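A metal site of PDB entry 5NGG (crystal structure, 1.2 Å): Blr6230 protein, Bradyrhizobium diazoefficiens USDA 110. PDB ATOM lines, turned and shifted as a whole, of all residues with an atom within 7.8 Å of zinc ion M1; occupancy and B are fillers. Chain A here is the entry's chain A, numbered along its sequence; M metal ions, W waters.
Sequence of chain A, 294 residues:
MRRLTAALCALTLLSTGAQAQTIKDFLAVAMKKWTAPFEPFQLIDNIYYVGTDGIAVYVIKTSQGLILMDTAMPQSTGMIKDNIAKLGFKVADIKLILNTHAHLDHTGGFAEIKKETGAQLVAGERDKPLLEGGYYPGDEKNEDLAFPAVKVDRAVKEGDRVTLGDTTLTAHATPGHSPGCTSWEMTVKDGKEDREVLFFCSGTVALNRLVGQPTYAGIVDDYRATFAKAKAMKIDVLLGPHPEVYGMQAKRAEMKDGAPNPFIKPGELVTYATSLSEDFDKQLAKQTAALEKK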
ATOM      1  N   PHE A  26     -15.124  -0.290 -24.917  1.00  0.00           N
ATOM      2  CA  PHE A  26     -14.272   0.238 -23.844  1.00  0.00           C
ATOM      3  C   PHE A  26     -12.993   0.842 -24.438  1.00  0.00           C
ATOM      4  O   PHE A  26     -12.620   1.967 -24.079  1.00  0.00           O
ATOM      5  CB  PHE A  26     -13.930  -0.863 -22.844  1.00  0.00           C
ATOM      6  CG  PHE A  26     -12.966  -0.449 -21.778  1.00  0.00           C
ATOM      7  CD1 PHE A  26     -11.587  -0.602 -21.963  1.00  0.00           C
ATOM      8  CD2 PHE A  26     -13.409   0.056 -20.576  1.00  0.00           C
ATOM      9  CE1 PHE A  26     -10.687  -0.234 -20.976  1.00  0.00           C
ATOM     10  CE2 PHE A  26     -12.512   0.417 -19.583  1.00  0.00           C
ATOM     11  CZ  PHE A  26     -11.157   0.279 -19.779  1.00  0.00           C
ATOM     12  N   TRP A  34     -10.896   9.568 -23.421  1.00  0.00           N
ATOM     13  CA  TRP A  34      -9.927   9.281 -22.424  1.00  0.00           C
ATOM     14  C   TRP A  34      -8.549   9.824 -22.728  1.00  0.00           C
ATOM     15  O   TRP A  34      -7.796  10.040 -21.804  1.00  0.00           O
ATOM     16  CB  TRP A  34      -9.883   7.794 -22.157  1.00  0.00           C
ATOM     17  CG  TRP A  34     -11.087   7.256 -21.397  1.00  0.00           C
ATOM     18  CD1 TRP A  34     -12.288   7.884 -21.206  1.00  0.00           C
ATOM     19  CD2 TRP A  34     -11.222   5.962 -20.780  1.00  0.00           C
ATOM     20  NE1 TRP A  34     -13.138   7.077 -20.488  1.00  0.00           N
ATOM     21  CE2 TRP A  34     -12.501   5.894 -20.216  1.00  0.00           C
ATOM     22  CE3 TRP A  34     -10.364   4.867 -20.648  1.00  0.00           C
ATOM     23  CZ2 TRP A  34     -12.961   4.780 -19.516  1.00  0.00           C
ATOM     24  CZ3 TRP A  34     -10.821   3.750 -19.965  1.00  0.00           C
ATOM     25  CH2 TRP A  34     -12.117   3.719 -19.415  1.00  0.00           C
ATOM     26  N   THR A 100      -5.704   4.434  -6.979  1.00  0.00           N
ATOM     27  CA  THR A 100      -7.073   4.073  -6.584  1.00  0.00           C
ATOM     28  C   THR A 100      -7.328   2.596  -6.925  1.00  0.00           C
ATOM     29  O   THR A 100      -7.715   1.802  -6.080  1.00  0.00           O
ATOM     30  CB  THR A 100      -8.138   4.933  -7.295  1.00  0.00           C
ATOM     31  OG1 THR A 100      -7.890   4.939  -8.705  1.00  0.00           O
ATOM     32  CG2 THR A 100      -8.175   6.335  -6.696  1.00  0.00           C
ATOM     33  N   HIS A 101      -7.103   2.211  -8.178  1.00  0.00           N
ATOM     34  CA  HIS A 101      -7.299   0.795  -8.549  1.00  0.00           C
ATOM     35  C   HIS A 101      -6.499   0.451  -9.794  1.00  0.00           C
ATOM     36  O   HIS A 101      -6.187   1.312 -10.619  1.00  0.00           O
ATOM     37  CB  HIS A 101      -8.774   0.429  -8.700  1.00  0.00           C
ATOM     38  CG  HIS A 101      -9.390   0.922  -9.973  1.00  0.00           C
ATOM     39  ND1 HIS A 101     -10.099   2.108 -10.061  1.00  0.00           N
ATOM     40  CD2 HIS A 101      -9.462   0.345 -11.187  1.00  0.00           C
ATOM     41  CE1 HIS A 101     -10.540   2.250 -11.300  1.00  0.00           C
ATOM     42  NE2 HIS A 101     -10.151   1.216 -12.015  1.00  0.00           N
ATOM     43  N   ALA A 102      -6.185  -0.828  -9.916  1.00  0.00           N
ATOM     44  CA  ALA A 102      -5.157  -1.292 -10.842  1.00  0.00           C
ATOM     45  C   ALA A 102      -5.712  -1.741 -12.196  1.00  0.00           C
ATOM     46  O   ALA A 102      -5.598  -2.907 -12.554  1.00  0.00           O
ATOM     47  CB  ALA A 102      -4.377  -2.407 -10.170  1.00  0.00           C
ATOM     48  N   HIS A 103      -6.271  -0.811 -12.960  1.00  0.00           N
ATOM     49  CA  HIS A 103      -6.626  -0.999 -14.372  1.00  0.00           C
ATOM     50  C   HIS A 103      -5.810  -0.055 -15.223  1.00  0.00           C
ATOM     51  O   HIS A 103      -5.410   1.022 -14.763  1.00  0.00           O
ATOM     52  CB  HIS A 103      -8.113  -0.726 -14.618  1.00  0.00           C
ATOM     53  CG  HIS A 103      -9.034  -1.714 -14.017  1.00  0.00           C
ATOM     54  ND1 HIS A 103     -10.344  -1.418 -13.756  1.00  0.00           N
ATOM     55  CD2 HIS A 103      -8.854  -3.006 -13.649  1.00  0.00           C
ATOM     56  CE1 HIS A 103     -10.944  -2.481 -13.268  1.00  0.00           C
ATOM     57  NE2 HIS A 103     -10.060  -3.462 -13.185  1.00  0.00           N
ATOM     58  N   LEU A 104      -5.558  -0.467 -16.462  1.00  0.00           N
ATOM     59  CA  LEU A 104      -4.623   0.253 -17.356  1.00  0.00           C
ATOM     60  C   LEU A 104      -4.939   1.724 -17.583  1.00  0.00           C
ATOM     61  O   LEU A 104      -4.028   2.482 -17.866  1.00  0.00           O
ATOM     62  CB  LEU A 104      -4.485  -0.437 -18.699  1.00  0.00           C
ATOM     63  CG  LEU A 104      -5.528  -0.185 -19.785  1.00  0.00           C
ATOM     64  CD1 LEU A 104      -5.009  -0.658 -21.146  1.00  0.00           C
ATOM     65  CD2 LEU A 104      -6.836  -0.861 -19.450  1.00  0.00           C
ATOM     66  N   ASP A 105      -6.213   2.123 -17.486  1.00  0.00           N
ATOM     67  CA  ASP A 105      -6.574   3.510 -17.672  1.00  0.00           C
ATOM     68  C   ASP A 105      -6.181   4.395 -16.498  1.00  0.00           C
ATOM     69  O   ASP A 105      -6.263   5.629 -16.607  1.00  0.00           O
ATOM     70  CB  ASP A 105      -8.061   3.671 -18.036  1.00  0.00           C
ATOM     71  CG  ASP A 105      -9.057   3.012 -17.090  1.00  0.00           C
ATOM     72  OD1 ASP A 105      -8.789   1.893 -16.588  1.00  0.00           O
ATOM     73  OD2 ASP A 105     -10.123   3.675 -16.891  1.00  0.00           O
ATOM     74  N   HIS A 106      -5.711   3.789 -15.401  1.00  0.00           N
ATOM     75  CA  HIS A 106      -5.216   4.520 -14.236  1.00  0.00           C
ATOM     76  C   HIS A 106      -3.755   4.214 -13.900  1.00  0.00           C
ATOM     77  O   HIS A 106      -3.136   4.958 -13.138  1.00  0.00           O
ATOM     78  CB  HIS A 106      -6.099   4.252 -13.021  1.00  0.00           C
ATOM     79  CG  HIS A 106      -7.558   4.444 -13.339  1.00  0.00           C
ATOM     80  ND1 HIS A 106      -8.088   5.680 -13.627  1.00  0.00           N
ATOM     81  CD2 HIS A 106      -8.537   3.554 -13.583  1.00  0.00           C
ATOM     82  CE1 HIS A 106      -9.342   5.533 -14.009  1.00  0.00           C
ATOM     83  NE2 HIS A 106      -9.655   4.247 -13.975  1.00  0.00           N
ATOM     84  N   TYR A 136      -5.232  -7.632 -16.528  1.00  0.00           N
ATOM     85  CA  TYR A 136      -6.611  -7.457 -16.075  1.00  0.00           C
ATOM     86  C   TYR A 136      -7.072  -8.741 -15.372  1.00  0.00           C
ATOM     87  O   TYR A 136      -6.986  -9.820 -15.972  1.00  0.00           O
ATOM     88  CB  TYR A 136      -7.538  -7.122 -17.263  1.00  0.00           C
ATOM     89  CG  TYR A 136      -8.850  -6.552 -16.802  1.00  0.00           C
ATOM     90  CD1 TYR A 136      -9.893  -7.376 -16.346  1.00  0.00           C
ATOM     91  CD2 TYR A 136      -9.053  -5.175 -16.739  1.00  0.00           C
ATOM     92  CE1 TYR A 136     -11.074  -6.848 -15.853  1.00  0.00           C
ATOM     93  CE2 TYR A 136     -10.241  -4.650 -16.252  1.00  0.00           C
ATOM     94  CZ  TYR A 136     -11.244  -5.473 -15.808  1.00  0.00           C
ATOM     95  OH  TYR A 136     -12.405  -4.906 -15.325  1.00  0.00           O
ATOM     96  N   HIS A 177     -14.892  -2.945  -7.867  1.00  0.00           N
ATOM     97  CA  HIS A 177     -14.445  -2.617  -9.209  1.00  0.00           C
ATOM     98  C   HIS A 177     -13.066  -3.276  -9.486  1.00  0.00           C
ATOM     99  O   HIS A 177     -12.775  -3.667 -10.623  1.00  0.00           O
ATOM    100  CB  HIS A 177     -14.435  -1.094  -9.396  1.00  0.00           C
ATOM    101  CG  HIS A 177     -14.015  -0.658 -10.759  1.00  0.00           C
ATOM    102  ND1 HIS A 177     -14.863  -0.586 -11.835  1.00  0.00           N
ATOM    103  CD2 HIS A 177     -12.796  -0.317 -11.215  1.00  0.00           C
ATOM    104  CE1 HIS A 177     -14.179  -0.176 -12.901  1.00  0.00           C
ATOM    105  NE2 HIS A 177     -12.920  -0.034 -12.553  1.00  0.00           N
ATOM    106  N   SER A 178     -12.217  -3.350  -8.457  1.00  0.00           N
ATOM    107  CA  SER A 178     -11.043  -4.223  -8.460  1.00  0.00           C
ATOM    108  C   SER A 178     -10.928  -4.799  -7.055  1.00  0.00           C
ATOM    109  O   SER A 178     -11.507  -4.258  -6.109  1.00  0.00           O
ATOM    110  CB  SER A 178      -9.769  -3.452  -8.833  1.00  0.00           C
ATOM    111  OG  SER A 178      -9.332  -2.633  -7.755  1.00  0.00           O
ATOM    112  N   CYS A 181      -9.226  -2.125  -4.741  1.00  0.00           N
ATOM    113  CA  CYS A 181      -9.696  -0.750  -4.959  1.00  0.00           C
ATOM    114  C   CYS A 181      -9.650   0.015  -3.618  1.00  0.00           C
ATOM    115  O   CYS A 181     -10.258  -0.463  -2.618  1.00  0.00           O
ATOM    116  CB  CYS A 181     -11.120  -0.845  -5.504  1.00  0.00           C
ATOM    117  SG  CYS A 181     -11.782   0.441  -6.599  1.00  0.00           S
ATOM    118  N   CYS A 201     -12.526   5.280  -5.368  1.00  0.00           N
ATOM    119  CA  CYS A 201     -11.758   4.465  -6.285  1.00  0.00           C
ATOM    120  C   CYS A 201     -12.431   4.026  -7.546  1.00  0.00           C
ATOM    121  O   CYS A 201     -11.713   3.574  -8.437  1.00  0.00           O
ATOM    122  CB  CYS A 201     -11.200   3.232  -5.550  1.00  0.00           C
ATOM    123  SG  CYS A 201     -12.386   1.939  -5.232  1.00  0.00           S
ATOM    124  N   SER A 202     -13.751   4.098  -7.588  1.00  0.00           N
ATOM    125  CA  SER A 202     -14.670   3.577  -8.654  1.00  0.00           C
ATOM    126  C   SER A 202     -15.546   2.483  -8.083  1.00  0.00           C
ATOM    127  O   SER A 202     -15.032   1.579  -7.436  1.00  0.00           O
ATOM    128  CB  SER A 202     -14.032   2.985  -9.902  1.00  0.00           C
ATOM    129  OG  SER A 202     -15.086   2.450 -10.708  1.00  0.00           O
ATOM    130  N   THR A 204     -18.121   1.212 -10.532  1.00  0.00           N
ATOM    131  CA  THR A 204     -18.838   0.798 -11.726  1.00  0.00           C
ATOM    132  C   THR A 204     -18.628  -0.698 -11.989  1.00  0.00           C
ATOM    133  O   THR A 204     -17.590  -1.260 -11.588  1.00  0.00           O
ATOM    134  CB  THR A 204     -18.372   1.581 -12.959  1.00  0.00           C
ATOM    135  OG1 THR A 204     -17.002   1.276 -13.156  1.00  0.00           O
ATOM    136  CG2 THR A 204     -18.586   3.091 -12.805  1.00  0.00           C
ATOM    137  N   VAL A 205     -19.579  -1.336 -12.658  1.00  0.00           N
ATOM    138  CA  VAL A 205     -19.408  -2.713 -13.104  1.00  0.00           C
ATOM    139  C   VAL A 205     -18.416  -2.809 -14.270  1.00  0.00           C
ATOM    140  O   VAL A 205     -17.528  -3.672 -14.276  1.00  0.00           O
ATOM    141  CB  VAL A 205     -20.757  -3.358 -13.447  1.00  0.00           C
ATOM    142  CG1 VAL A 205     -20.566  -4.736 -14.038  1.00  0.00           C
ATOM    143  CG2 VAL A 205     -21.616  -3.469 -12.176  1.00  0.00           C
ATOM    144  N   ALA A 206     -18.588  -1.930 -15.259  1.00  0.00           N
ATOM    145  CA  ALA A 206     -17.666  -1.783 -16.384  1.00  0.00           C
ATOM    146  C   ALA A 206     -17.430  -3.165 -17.021  1.00  0.00           C
ATOM    147  O   ALA A 206     -18.424  -3.799 -17.413  1.00  0.00           O
ATOM    148  CB  ALA A 206     -16.394  -1.068 -15.927  1.00  0.00           C
ATOM    149  N   LEU A 207     -16.188  -3.632 -17.159  1.00  0.00           N
ATOM    150  CA  LEU A 207     -15.873  -4.884 -17.834  1.00  0.00           C
ATOM    151  C   LEU A 207     -15.947  -6.098 -16.919  1.00  0.00           C
ATOM    152  O   LEU A 207     -15.697  -7.212 -17.371  1.00  0.00           O
ATOM    153  CB  LEU A 207     -14.485  -4.826 -18.481  1.00  0.00           C
ATOM    154  CG  LEU A 207     -14.296  -3.760 -19.545  1.00  0.00           C
ATOM    155  CD1 LEU A 207     -12.868  -3.843 -20.046  1.00  0.00           C
ATOM    156  CD2 LEU A 207     -15.309  -3.913 -20.693  1.00  0.00           C
ATOM    157  N   ASN A 208     -16.236  -5.931 -15.636  1.00  0.00           N
ATOM    158  CA  ASN A 208     -16.199  -7.066 -14.722  1.00  0.00           C
ATOM    159  C   ASN A 208     -17.337  -8.067 -14.914  1.00  0.00           C
ATOM    160  O   ASN A 208     -18.470  -7.691 -15.235  1.00  0.00           O
ATOM    161  CB  ASN A 208     -16.197  -6.589 -13.278  1.00  0.00           C
ATOM    162  CG  ASN A 208     -14.909  -5.901 -12.904  1.00  0.00           C
ATOM    163  OD1 ASN A 208     -13.815  -6.219 -13.430  1.00  0.00           O
ATOM    164  ND2 ASN A 208     -14.995  -4.973 -11.973  1.00  0.00           N
ATOM    165  N   PRO A 241     -11.640   8.631 -10.177  1.00  0.00           N
ATOM    166  CA  PRO A 241     -10.629   8.417 -11.216  1.00  0.00           C
ATOM    167  C   PRO A 241     -11.108   8.707 -12.637  1.00  0.00           C
ATOM    168  O   PRO A 241     -10.297   8.656 -13.566  1.00  0.00           O
ATOM    169  CB  PRO A 241     -10.211   6.972 -11.019  1.00  0.00           C
ATOM    170  CG  PRO A 241     -11.380   6.317 -10.412  1.00  0.00           C
ATOM    171  CD  PRO A 241     -12.181   7.357  -9.671  1.00  0.00           C
ATOM    172  N   HIS A 242     -12.390   9.064 -12.789  1.00  0.00           N
ATOM    173  CA  HIS A 242     -12.945   9.585 -14.032  1.00  0.00           C
ATOM    174  C   HIS A 242     -13.744  10.824 -13.646  1.00  0.00           C
ATOM    175  O   HIS A 242     -14.434  10.812 -12.619  1.00  0.00           O
ATOM    176  CB  HIS A 242     -13.840   8.547 -14.732  1.00  0.00           C
ATOM    177  CG  HIS A 242     -13.092   7.349 -15.220  1.00  0.00           C
ATOM    178  ND1 HIS A 242     -12.353   7.339 -16.384  1.00  0.00           N
ATOM    179  CD2 HIS A 242     -12.970   6.117 -14.693  1.00  0.00           C
ATOM    180  CE1 HIS A 242     -11.819   6.130 -16.543  1.00  0.00           C
ATOM    181  NE2 HIS A 242     -12.168   5.378 -15.528  1.00  0.00           N
HETATM  182 ZN    ZN M   1     -11.217   0.460 -13.616  1.00  0.00          ZN
HETATM  183 ZN    ZN M   2     -11.227   3.534 -15.079  1.00  0.00          ZN
HETATM  184  O   HOH W   1     -12.893  -0.113 -16.369  1.00  0.00           O
HETATM  185  O   HOH W   2     -11.118   1.484 -15.165  1.00  0.00           O
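A ring nitrogen (ND1) of His 177 lies within hydrogen-bond range of the side-chain hydroxyl (OG) of Ser 202, 3.2 Å away. OH of Tyr 136 sits close to NE2 of His 103 (3.5 Å). O of His 177 is in hydrogen-bond range of ND2 of Asn 208. A ring nitrogen (ND1) of His 177 lies within hydrogen-bond range of the backbone carbonyl oxygen of Thr 204. A ring nitrogen (ND1) of His 101 lies within hydrogen-bond range of the backbone carbonyl oxygen of Cys 201. The side-chain sulfur of Cys 181 is disulfide-bonded to the side-chain sulfur of Cys 201 (2.1 Å).
Zinc ion M1 is bound by water W2 (1.9 Å), NE2 of His 101 (2.1 Å), NE2 of His 177 (2.1 Å) and ND1 of His 103 (2.1 Å).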
